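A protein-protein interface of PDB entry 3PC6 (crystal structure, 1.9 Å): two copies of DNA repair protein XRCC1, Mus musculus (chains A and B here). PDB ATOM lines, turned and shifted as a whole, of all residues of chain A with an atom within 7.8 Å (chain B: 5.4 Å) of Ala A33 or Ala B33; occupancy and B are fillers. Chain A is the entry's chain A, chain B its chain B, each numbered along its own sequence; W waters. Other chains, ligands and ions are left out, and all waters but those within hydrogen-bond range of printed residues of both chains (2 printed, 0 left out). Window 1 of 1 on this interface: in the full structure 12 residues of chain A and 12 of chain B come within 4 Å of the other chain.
The backbone carbonyl oxygen (O) of Pro A5 lies within hydrogen-bond range of the guanidinium group (NH2) of Arg B29, 3.0 Å away.
The guanidinium group (NH2) of Arg A29 sits at hydrogen-bond distance from the backbone carbonyl oxygen (O) of Pro B5.
The guanidinium group of Arg A29 sits at hydrogen-bond distance from the backbone carbonyl oxygen of Ala B33 (2.9 Å).
O of Ala A33 lies within hydrogen-bond range of NH2 of Arg B29, at 3.0 Å.
The side-chain hydroxyl (OG1) of Thr A32 lies within hydrogen-bond range of the backbone carbonyl oxygen (O) of Ile A28 (2.7 Å).
OG1 of Thr B32 lies within hydrogen-bond range of O of Ile B28 (2.7 Å).
CD2 of Leu B4 touches CD2 of Leu A4, at 3.6 Å.
NH2 of Arg B29 touches CB of Leu A4, at 3.6 Å.
Leu A4 touches Tyr B30.
CD1 of Leu A4 touches CB of Ala B33 (3.8 Å).
CD1 of Tyr A30 touches CD1 of Leu B4, at 3.8 Å.
Thr A32 touches Arg B29.
Thr B32 touches Thr A32 (CB to CG2, 3.8 Å).
Leu B4 touches Ala A33 (CD1 to CB, 3.9 Å).
Ala B33 touches Ala A33 (CB to CB, 3.7 Å).
Asn A35 touches Arg B29 (CG to NH1, 3.6 Å).
Arg A26 touches none of the printed residues of chain B.
Of the printed residues of chain B, Tyr A30 touches Leu B4 (3.8 Å).
Ala A33 touches just these residues of chain B: Leu B4, Arg B29 and Ala B33.
Of the printed residues of chain B, Asn A35 touches Arg B29 (3.6 Å).
Of the printed residues of chain A, Arg B29 touches Leu A4, Pro A5, Asp A6, Thr A32, Ala A33 and Asn A35.
Of the printed residues of chain A, Thr B32 touches Arg A29 and Thr A32.
Ala B33 touches just these residues of chain A: Leu A4 (3.8 Å), Arg A29 (2.9 Å) and Ala A33 (3.7 Å).
Of the 19 printed residues of chain A, 8 touch a printed residue of chain B.
Printed residues of chain A that touch a printed residue of chain B: Leu A4, Pro A5, Asp A6, Arg A29, Tyr A30, Thr A32, Ala A33 and Asn A35.
Hydrophobic or aromatic side chains of chain B within 4 Å of the printed part of chain A: Leu B4, Tyr B30 and Ala B33.
Among the printed residues, 18 pairs touch across the chains.
Leu B4 touches its own counterpart, Leu A4.
Leu A4 touches Arg B29, and with the chains exchanged Arg A29 touches Leu B4.
Arg A29 touches Thr B32, and with the chains exchanged Thr A32 touches Arg B29.
Arg A29 touches Asn B35, and with the chains exchanged Asn A35 touches Arg B29.
Positions printed for both chains: 4, 5, 28, 29, 30, 31, 32, 33, 34 and 35.
Of the 18 pairs that touch across the chains among the printed residues, 17 have their exchanged pair printed and touching as well.
Water W1 bridges OD1 of Asn A81 (2.6 Å) and N of Leu B4 (2.7 Å).
Water W2 lies within hydrogen-bond range of the backbone carbonyl oxygen of Leu A4 (2.8 Å), the side-chain carboxylate of Asp A6 (3.0 Å) and the guanidinium group of Arg B29 (3.1 Å).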
ATOM      1  N   GLU A   3      17.814 -15.464 -12.373  1.00  0.00           N
ATOM      2  CA  GLU A   3      19.092 -14.781 -12.204  1.00  0.00           C
ATOM      3  C   GLU A   3      20.106 -15.647 -11.452  1.00  0.00           C
ATOM      4  O   GLU A   3      19.828 -16.801 -11.121  1.00  0.00           O
ATOM      5  CB  GLU A   3      18.903 -13.448 -11.480  1.00  0.00           C
ATOM      6  CG  GLU A   3      18.405 -13.593 -10.055  1.00  0.00           C
ATOM      7  CD  GLU A   3      18.563 -12.321  -9.251  1.00  0.00           C
ATOM      8  OE1 GLU A   3      17.747 -12.095  -8.332  1.00  0.00           O
ATOM      9  OE2 GLU A   3      19.501 -11.546  -9.538  1.00  0.00           O
ATOM     10  N   LEU A   4      21.277 -15.077 -11.179  1.00  0.00           N
ATOM     11  CA  LEU A   4      22.380 -15.831 -10.591  1.00  0.00           C
ATOM     12  C   LEU A   4      22.254 -15.973  -9.079  1.00  0.00           C
ATOM     13  O   LEU A   4      22.065 -14.983  -8.362  1.00  0.00           O
ATOM     14  CB  LEU A   4      23.724 -15.176 -10.919  1.00  0.00           C
ATOM     15  CG  LEU A   4      24.236 -15.175 -12.363  1.00  0.00           C
ATOM     16  CD1 LEU A   4      25.456 -14.291 -12.449  1.00  0.00           C
ATOM     17  CD2 LEU A   4      24.570 -16.581 -12.835  1.00  0.00           C
ATOM     18  N   PRO A   5      22.394 -17.211  -8.590  1.00  0.00           N
ATOM     19  CA  PRO A   5      22.411 -17.484  -7.150  1.00  0.00           C
ATOM     20  C   PRO A   5      23.576 -16.738  -6.519  1.00  0.00           C
ATOM     21  O   PRO A   5      24.613 -16.573  -7.169  1.00  0.00           O
ATOM     22  CB  PRO A   5      22.673 -18.991  -7.081  1.00  0.00           C
ATOM     23  CG  PRO A   5      22.367 -19.515  -8.453  1.00  0.00           C
ATOM     24  CD  PRO A   5      22.697 -18.408  -9.388  1.00  0.00           C
ATOM     25  N   ASP A   6      23.420 -16.284  -5.281  1.00  0.00           N
ATOM     26  CA  ASP A   6      24.510 -15.580  -4.619  1.00  0.00           C
ATOM     27  C   ASP A   6      24.859 -16.220  -3.285  1.00  0.00           C
ATOM     28  O   ASP A   6      25.120 -15.534  -2.300  1.00  0.00           O
ATOM     29  CB  ASP A   6      24.192 -14.090  -4.462  1.00  0.00           C
ATOM     30  CG  ASP A   6      22.797 -13.837  -3.931  1.00  0.00           C
ATOM     31  OD1 ASP A   6      22.454 -14.381  -2.858  1.00  0.00           O
ATOM     32  OD2 ASP A   6      22.047 -13.075  -4.582  1.00  0.00           O
ATOM     33  N   PHE A   7      24.873 -17.547  -3.261  1.00  0.00           N
ATOM     34  CA  PHE A   7      25.045 -18.258  -2.002  1.00  0.00           C
ATOM     35  C   PHE A   7      26.492 -18.293  -1.496  1.00  0.00           C
ATOM     36  O   PHE A   7      26.738 -18.712  -0.366  1.00  0.00           O
ATOM     37  CB  PHE A   7      24.421 -19.661  -2.064  1.00  0.00           C
ATOM     38  CG  PHE A   7      24.896 -20.494  -3.215  1.00  0.00           C
ATOM     39  CD1 PHE A   7      26.150 -21.076  -3.190  1.00  0.00           C
ATOM     40  CD2 PHE A   7      24.076 -20.721  -4.308  1.00  0.00           C
ATOM     41  CE1 PHE A   7      26.587 -21.855  -4.241  1.00  0.00           C
ATOM     42  CE2 PHE A   7      24.505 -21.499  -5.366  1.00  0.00           C
ATOM     43  CZ  PHE A   7      25.765 -22.068  -5.332  1.00  0.00           C
ATOM     44  N   PHE A   8      27.437 -17.838  -2.320  1.00  0.00           N
ATOM     45  CA  PHE A   8      28.815 -17.628  -1.860  1.00  0.00           C
ATOM     46  C   PHE A   8      29.086 -16.190  -1.438  1.00  0.00           C
ATOM     47  O   PHE A   8      30.224 -15.844  -1.103  1.00  0.00           O
ATOM     48  CB  PHE A   8      29.826 -18.007  -2.942  1.00  0.00           C
ATOM     49  CG  PHE A   8      29.995 -19.474  -3.113  1.00  0.00           C
ATOM     50  CD1 PHE A   8      29.696 -20.340  -2.075  1.00  0.00           C
ATOM     51  CD2 PHE A   8      30.446 -19.999  -4.312  1.00  0.00           C
ATOM     52  CE1 PHE A   8      29.849 -21.708  -2.234  1.00  0.00           C
ATOM     53  CE2 PHE A   8      30.605 -21.364  -4.466  1.00  0.00           C
ATOM     54  CZ  PHE A   8      30.306 -22.218  -3.419  1.00  0.00           C
ATOM     55  N   ARG A  26      37.311 -23.663 -14.110  1.00  0.00           N
ATOM     56  CA  ARG A  26      35.960 -24.049 -13.683  1.00  0.00           C
ATOM     57  C   ARG A  26      35.652 -23.594 -12.260  1.00  0.00           C
ATOM     58  O   ARG A  26      34.574 -23.062 -11.983  1.00  0.00           O
ATOM     59  CB  ARG A  26      35.755 -25.569 -13.767  1.00  0.00           C
ATOM     60  CG  ARG A  26      35.192 -26.058 -15.080  1.00  0.00           C
ATOM     61  CD  ARG A  26      34.673 -27.484 -14.956  1.00  0.00           C
ATOM     62  NE  ARG A  26      35.673 -28.385 -14.392  1.00  0.00           N
ATOM     63  CZ  ARG A  26      36.623 -28.982 -15.101  1.00  0.00           C
ATOM     64  NH1 ARG A  26      36.708 -28.768 -16.406  1.00  0.00           N
ATOM     65  NH2 ARG A  26      37.493 -29.787 -14.504  1.00  0.00           N
ATOM     66  N   LEU A  27      36.586 -23.837 -11.344  1.00  0.00           N
ATOM     67  CA  LEU A  27      36.400 -23.404  -9.964  1.00  0.00           C
ATOM     68  C   LEU A  27      36.231 -21.885  -9.873  1.00  0.00           C
ATOM     69  O   LEU A  27      35.354 -21.385  -9.164  1.00  0.00           O
ATOM     70  CB  LEU A  27      37.570 -23.859  -9.081  1.00  0.00           C
ATOM     71  CG  LEU A  27      37.694 -25.367  -8.838  1.00  0.00           C
ATOM     72  CD1 LEU A  27      38.928 -25.675  -7.996  1.00  0.00           C
ATOM     73  CD2 LEU A  27      36.452 -25.900  -8.134  1.00  0.00           C
ATOM     74  N   ILE A  28      37.085 -21.155 -10.581  1.00  0.00           N
ATOM     75  CA  ILE A  28      36.972 -19.698 -10.620  1.00  0.00           C
ATOM     76  C   ILE A  28      35.606 -19.309 -11.151  1.00  0.00           C
ATOM     77  O   ILE A  28      34.938 -18.431 -10.607  1.00  0.00           O
ATOM     78  CB  ILE A  28      38.085 -19.068 -11.481  1.00  0.00           C
ATOM     79  CG1 ILE A  28      39.439 -19.240 -10.783  1.00  0.00           C
ATOM     80  CG2 ILE A  28      37.789 -17.591 -11.750  1.00  0.00           C
ATOM     81  CD1 ILE A  28      40.633 -18.934 -11.680  1.00  0.00           C
ATOM     82  N   ARG A  29      35.169 -19.989 -12.205  1.00  0.00           N
ATOM     83  CA  ARG A  29      33.871 -19.677 -12.772  1.00  0.00           C
ATOM     84  C   ARG A  29      32.738 -19.780 -11.755  1.00  0.00           C
ATOM     85  O   ARG A  29      31.951 -18.849 -11.622  1.00  0.00           O
ATOM     86  CB  ARG A  29      33.569 -20.533 -14.003  1.00  0.00           C
ATOM     87  CG  ARG A  29      32.261 -20.119 -14.671  1.00  0.00           C
ATOM     88  CD  ARG A  29      31.955 -20.966 -15.893  1.00  0.00           C
ATOM     89  NE  ARG A  29      30.670 -20.583 -16.467  1.00  0.00           N
ATOM     90  CZ  ARG A  29      30.019 -21.298 -17.378  1.00  0.00           C
ATOM     91  NH1 ARG A  29      30.532 -22.442 -17.808  1.00  0.00           N
ATOM     92  NH2 ARG A  29      28.855 -20.874 -17.847  1.00  0.00           N
ATOM     93  N   TYR A  30      32.656 -20.905 -11.038  1.00  0.00           N
ATOM     94  CA  TYR A  30      31.581 -21.118 -10.072  1.00  0.00           C
ATOM     95  C   TYR A  30      31.670 -20.202  -8.852  1.00  0.00           C
ATOM     96  O   TYR A  30      30.662 -19.666  -8.396  1.00  0.00           O
ATOM     97  CB  TYR A  30      31.549 -22.579  -9.607  1.00  0.00           C
ATOM     98  CG  TYR A  30      31.302 -23.559 -10.732  1.00  0.00           C
ATOM     99  CD1 TYR A  30      30.290 -23.341 -11.653  1.00  0.00           C
ATOM    100  CD2 TYR A  30      32.073 -24.706 -10.862  1.00  0.00           C
ATOM    101  CE1 TYR A  30      30.060 -24.229 -12.684  1.00  0.00           C
ATOM    102  CE2 TYR A  30      31.846 -25.605 -11.889  1.00  0.00           C
ATOM    103  CZ  TYR A  30      30.840 -25.362 -12.795  1.00  0.00           C
ATOM    104  OH  TYR A  30      30.612 -26.258 -13.819  1.00  0.00           O
ATOM    105  N   VAL A  31      32.866 -20.039  -8.304  1.00  0.00           N
ATOM    106  CA  VAL A  31      33.012 -19.205  -7.121  1.00  0.00           C
ATOM    107  C   VAL A  31      32.585 -17.774  -7.471  1.00  0.00           C
ATOM    108  O   VAL A  31      31.818 -17.136  -6.744  1.00  0.00           O
ATOM    109  CB  VAL A  31      34.458 -19.228  -6.568  1.00  0.00           C
ATOM    110  CG1 VAL A  31      34.638 -18.165  -5.507  1.00  0.00           C
ATOM    111  CG2 VAL A  31      34.796 -20.604  -5.993  1.00  0.00           C
ATOM    112  N   THR A  32      33.067 -17.291  -8.606  1.00  0.00           N
ATOM    113  CA  THR A  32      32.741 -15.944  -9.063  1.00  0.00           C
ATOM    114  C   THR A  32      31.235 -15.782  -9.349  1.00  0.00           C
ATOM    115  O   THR A  32      30.606 -14.819  -8.903  1.00  0.00           O
ATOM    116  CB  THR A  32      33.545 -15.617 -10.336  1.00  0.00           C
ATOM    117  OG1 THR A  32      34.950 -15.771 -10.065  1.00  0.00           O
ATOM    118  CG2 THR A  32      33.263 -14.189 -10.810  1.00  0.00           C
ATOM    119  N   ALA A  33      30.672 -16.736 -10.084  1.00  0.00           N
ATOM    120  CA  ALA A  33      29.266 -16.702 -10.477  1.00  0.00           C
ATOM    121  C   ALA A  33      28.324 -16.623  -9.288  1.00  0.00           C
ATOM    122  O   ALA A  33      27.296 -15.955  -9.356  1.00  0.00           O
ATOM    123  CB  ALA A  33      28.922 -17.914 -11.348  1.00  0.00           C
ATOM    124  N   PHE A  34      28.664 -17.306  -8.196  1.00  0.00           N
ATOM    125  CA  PHE A  34      27.772 -17.344  -7.044  1.00  0.00           C
ATOM    126  C   PHE A  34      28.168 -16.299  -6.028  1.00  0.00           C
ATOM    127  O   PHE A  34      27.779 -16.356  -4.858  1.00  0.00           O
ATOM    128  CB  PHE A  34      27.714 -18.750  -6.451  1.00  0.00           C
ATOM    129  CG  PHE A  34      27.411 -19.811  -7.475  1.00  0.00           C
ATOM    130  CD1 PHE A  34      26.426 -19.604  -8.429  1.00  0.00           C
ATOM    131  CD2 PHE A  34      28.111 -21.004  -7.491  1.00  0.00           C
ATOM    132  CE1 PHE A  34      26.143 -20.569  -9.386  1.00  0.00           C
ATOM    133  CE2 PHE A  34      27.832 -21.976  -8.441  1.00  0.00           C
ATOM    134  CZ  PHE A  34      26.845 -21.757  -9.392  1.00  0.00           C
ATOM    135  N   ASN A  35      28.955 -15.340  -6.509  1.00  0.00           N
ATOM    136  CA  ASN A  35      29.267 -14.121  -5.783  1.00  0.00           C
ATOM    137  C   ASN A  35      30.303 -14.287  -4.679  1.00  0.00           C
ATOM    138  O   ASN A  35      30.337 -13.500  -3.731  1.00  0.00           O
ATOM    139  CB  ASN A  35      27.997 -13.460  -5.238  1.00  0.00           C
ATOM    140  CG  ASN A  35      28.139 -11.961  -5.122  1.00  0.00           C
ATOM    141  OD1 ASN A  35      29.049 -11.373  -5.706  1.00  0.00           O
ATOM    142  ND2 ASN A  35      27.246 -11.331  -4.368  1.00  0.00           N
ATOM    143  N   GLY A  36      31.149 -15.303  -4.816  1.00  0.00           N
ATOM    144  CA  GLY A  36      32.247 -15.510  -3.888  1.00  0.00           C
ATOM    145  C   GLY A  36      33.376 -14.550  -4.226  1.00  0.00           C
ATOM    146  O   GLY A  36      33.387 -13.950  -5.298  1.00  0.00           O
ATOM    147  N   LEU A  38      37.529 -14.181  -4.611  1.00  0.00           N
ATOM    148  CA  LEU A  38      38.783 -14.918  -4.745  1.00  0.00           C
ATOM    149  C   LEU A  38      39.996 -14.088  -4.340  1.00  0.00           C
ATOM    150  O   LEU A  38      40.192 -12.993  -4.851  1.00  0.00           O
ATOM    151  CB  LEU A  38      38.939 -15.400  -6.185  1.00  0.00           C
ATOM    152  CG  LEU A  38      38.026 -16.580  -6.529  1.00  0.00           C
ATOM    153  CD1 LEU A  38      37.738 -16.628  -8.012  1.00  0.00           C
ATOM    154  CD2 LEU A  38      38.632 -17.885  -6.046  1.00  0.00           C
ATOM    155  N   ASN A  81      27.188 -26.223  -7.169  1.00  0.00           N
ATOM    156  CA  ASN A  81      26.669 -25.890  -8.486  1.00  0.00           C
ATOM    157  C   ASN A  81      25.565 -26.844  -8.911  1.00  0.00           C
ATOM    158  O   ASN A  81      24.486 -26.416  -9.323  1.00  0.00           O
ATOM    159  CB  ASN A  81      27.772 -25.881  -9.534  1.00  0.00           C
ATOM    160  CG  ASN A  81      27.234 -25.563 -10.917  1.00  0.00           C
ATOM    161  OD1 ASN A  81      26.562 -24.551 -11.109  1.00  0.00           O
ATOM    162  ND2 ASN A  81      27.500 -26.438 -11.875  1.00  0.00           N
ATOM    163  N   LEU B   4      24.517 -22.912 -15.601  1.00  0.00           N
ATOM    164  CA  LEU B   4      25.008 -21.604 -16.026  1.00  0.00           C
ATOM    165  C   LEU B   4      24.982 -21.495 -17.547  1.00  0.00           C
ATOM    166  O   LEU B   4      25.510 -22.368 -18.249  1.00  0.00           O
ATOM    167  CB  LEU B   4      26.436 -21.349 -15.523  1.00  0.00           C
ATOM    168  CG  LEU B   4      26.672 -21.097 -14.028  1.00  0.00           C
ATOM    169  CD1 LEU B   4      28.164 -20.911 -13.739  1.00  0.00           C
ATOM    170  CD2 LEU B   4      25.869 -19.894 -13.534  1.00  0.00           C
ATOM    171  N   PRO B   5      24.365 -20.420 -18.061  1.00  0.00           N
ATOM    172  CA  PRO B   5      24.368 -20.155 -19.502  1.00  0.00           C
ATOM    173  C   PRO B   5      25.790 -19.969 -20.019  1.00  0.00           C
ATOM    174  O   PRO B   5      26.672 -19.590 -19.250  1.00  0.00           O
ATOM    175  CB  PRO B   5      23.581 -18.847 -19.617  1.00  0.00           C
ATOM    176  CG  PRO B   5      22.711 -18.822 -18.416  1.00  0.00           C
ATOM    177  CD  PRO B   5      23.514 -19.472 -17.323  1.00  0.00           C
ATOM    178  N   ILE B  28      32.785  -8.264 -13.964  1.00  0.00           N
ATOM    179  CA  ILE B  28      33.626  -9.451 -13.895  1.00  0.00           C
ATOM    180  C   ILE B  28      32.747 -10.669 -13.603  1.00  0.00           C
ATOM    181  O   ILE B  28      32.908 -11.716 -14.215  1.00  0.00           O
ATOM    182  CB  ILE B  28      34.705  -9.301 -12.808  1.00  0.00           C
ATOM    183  CG1 ILE B  28      35.775  -8.305 -13.261  1.00  0.00           C
ATOM    184  CG2 ILE B  28      35.353 -10.634 -12.509  1.00  0.00           C
ATOM    185  CD1 ILE B  28      36.668  -7.814 -12.096  1.00  0.00           C
ATOM    186  N   ARG B  29      31.803 -10.515 -12.681  1.00  0.00           N
ATOM    187  CA  ARG B  29      30.904 -11.611 -12.311  1.00  0.00           C
ATOM    188  C   ARG B  29      30.081 -12.146 -13.483  1.00  0.00           C
ATOM    189  O   ARG B  29      30.036 -13.356 -13.710  1.00  0.00           O
ATOM    190  CB  ARG B  29      29.980 -11.194 -11.164  1.00  0.00           C
ATOM    191  CG  ARG B  29      29.083 -12.300 -10.654  1.00  0.00           C
ATOM    192  CD  ARG B  29      28.171 -11.822  -9.530  1.00  0.00           C
ATOM    193  NE  ARG B  29      27.308 -12.917  -9.114  1.00  0.00           N
ATOM    194  CZ  ARG B  29      26.234 -12.806  -8.339  1.00  0.00           C
ATOM    195  NH1 ARG B  29      25.861 -11.626  -7.865  1.00  0.00           N
ATOM    196  NH2 ARG B  29      25.533 -13.894  -8.036  1.00  0.00           N
ATOM    197  N   TYR B  30      29.428 -11.250 -14.224  1.00  0.00           N
ATOM    198  CA  TYR B  30      28.584 -11.670 -15.346  1.00  0.00           C
ATOM    199  C   TYR B  30      29.404 -12.211 -16.508  1.00  0.00           C
ATOM    200  O   TYR B  30      29.077 -13.251 -17.080  1.00  0.00           O
ATOM    201  CB  TYR B  30      27.707 -10.525 -15.839  1.00  0.00           C
ATOM    202  CG  TYR B  30      26.681 -10.047 -14.842  1.00  0.00           C
ATOM    203  CD1 TYR B  30      26.286 -10.846 -13.782  1.00  0.00           C
ATOM    204  CD2 TYR B  30      26.099  -8.789 -14.972  1.00  0.00           C
ATOM    205  CE1 TYR B  30      25.345 -10.400 -12.859  1.00  0.00           C
ATOM    206  CE2 TYR B  30      25.157  -8.335 -14.068  1.00  0.00           C
ATOM    207  CZ  TYR B  30      24.782  -9.143 -13.013  1.00  0.00           C
ATOM    208  OH  TYR B  30      23.840  -8.682 -12.117  1.00  0.00           O
ATOM    209  N   VAL B  31      30.463 -11.502 -16.875  1.00  0.00           N
ATOM    210  CA  VAL B  31      31.317 -11.987 -17.950  1.00  0.00           C
ATOM    211  C   VAL B  31      31.779 -13.404 -17.615  1.00  0.00           C
ATOM    212  O   VAL B  31      31.656 -14.315 -18.432  1.00  0.00           O
ATOM    213  CB  VAL B  31      32.539 -11.097 -18.155  1.00  0.00           C
ATOM    214  CG1 VAL B  31      33.528 -11.783 -19.082  1.00  0.00           C
ATOM    215  CG2 VAL B  31      32.119  -9.729 -18.728  1.00  0.00           C
ATOM    216  N   THR B  32      32.306 -13.578 -16.407  1.00  0.00           N
ATOM    217  CA  THR B  32      32.823 -14.880 -15.975  1.00  0.00           C
ATOM    218  C   THR B  32      31.718 -15.937 -15.901  1.00  0.00           C
ATOM    219  O   THR B  32      31.898 -17.057 -16.371  1.00  0.00           O
ATOM    220  CB  THR B  32      33.522 -14.787 -14.601  1.00  0.00           C
ATOM    221  OG1 THR B  32      34.540 -13.783 -14.644  1.00  0.00           O
ATOM    222  CG2 THR B  32      34.163 -16.133 -14.219  1.00  0.00           C
ATOM    223  N   ALA B  33      30.580 -15.576 -15.309  1.00  0.00           N
ATOM    224  CA  ALA B  33      29.494 -16.539 -15.109  1.00  0.00           C
ATOM    225  C   ALA B  33      29.006 -17.134 -16.425  1.00  0.00           C
ATOM    226  O   ALA B  33      28.618 -18.296 -16.472  1.00  0.00           O
ATOM    227  CB  ALA B  33      28.340 -15.911 -14.350  1.00  0.00           C
ATOM    228  N   PHE B  34      29.038 -16.342 -17.495  1.00  0.00           N
ATOM    229  CA  PHE B  34      28.502 -16.804 -18.780  1.00  0.00           C
ATOM    230  C   PHE B  34      29.608 -17.293 -19.704  1.00  0.00           C
ATOM    231  O   PHE B  34      29.476 -17.297 -20.929  1.00  0.00           O
ATOM    232  CB  PHE B  34      27.640 -15.720 -19.414  1.00  0.00           C
ATOM    233  CG  PHE B  34      26.551 -15.228 -18.504  1.00  0.00           C
ATOM    234  CD1 PHE B  34      25.789 -16.126 -17.781  1.00  0.00           C
ATOM    235  CD2 PHE B  34      26.307 -13.876 -18.348  1.00  0.00           C
ATOM    236  CE1 PHE B  34      24.792 -15.687 -16.928  1.00  0.00           C
ATOM    237  CE2 PHE B  34      25.312 -13.434 -17.498  1.00  0.00           C
ATOM    238  CZ  PHE B  34      24.555 -14.341 -16.786  1.00  0.00           C
ATOM    239  N   ASN B  35      30.705 -17.710 -19.080  1.00  0.00           N
ATOM    240  CA  ASN B  35      31.817 -18.369 -19.756  1.00  0.00           C
ATOM    241  C   ASN B  35      32.676 -17.478 -20.641  1.00  0.00           C
ATOM    242  O   ASN B  35      33.430 -17.978 -21.472  1.00  0.00           O
ATOM    243  CB  ASN B  35      31.339 -19.596 -20.545  1.00  0.00           C
ATOM    244  CG  ASN B  35      32.301 -20.770 -20.429  1.00  0.00           C
ATOM    245  OD1 ASN B  35      33.307 -20.687 -19.726  1.00  0.00           O
ATOM    246  ND2 ASN B  35      31.990 -21.868 -21.113  1.00  0.00           N
HETATM  247  O   HOH W   1      25.240 -24.121 -13.253  1.00  0.00           O
HETATM  248  O   HOH W   2      22.838 -12.431  -7.378  1.00  0.00           O
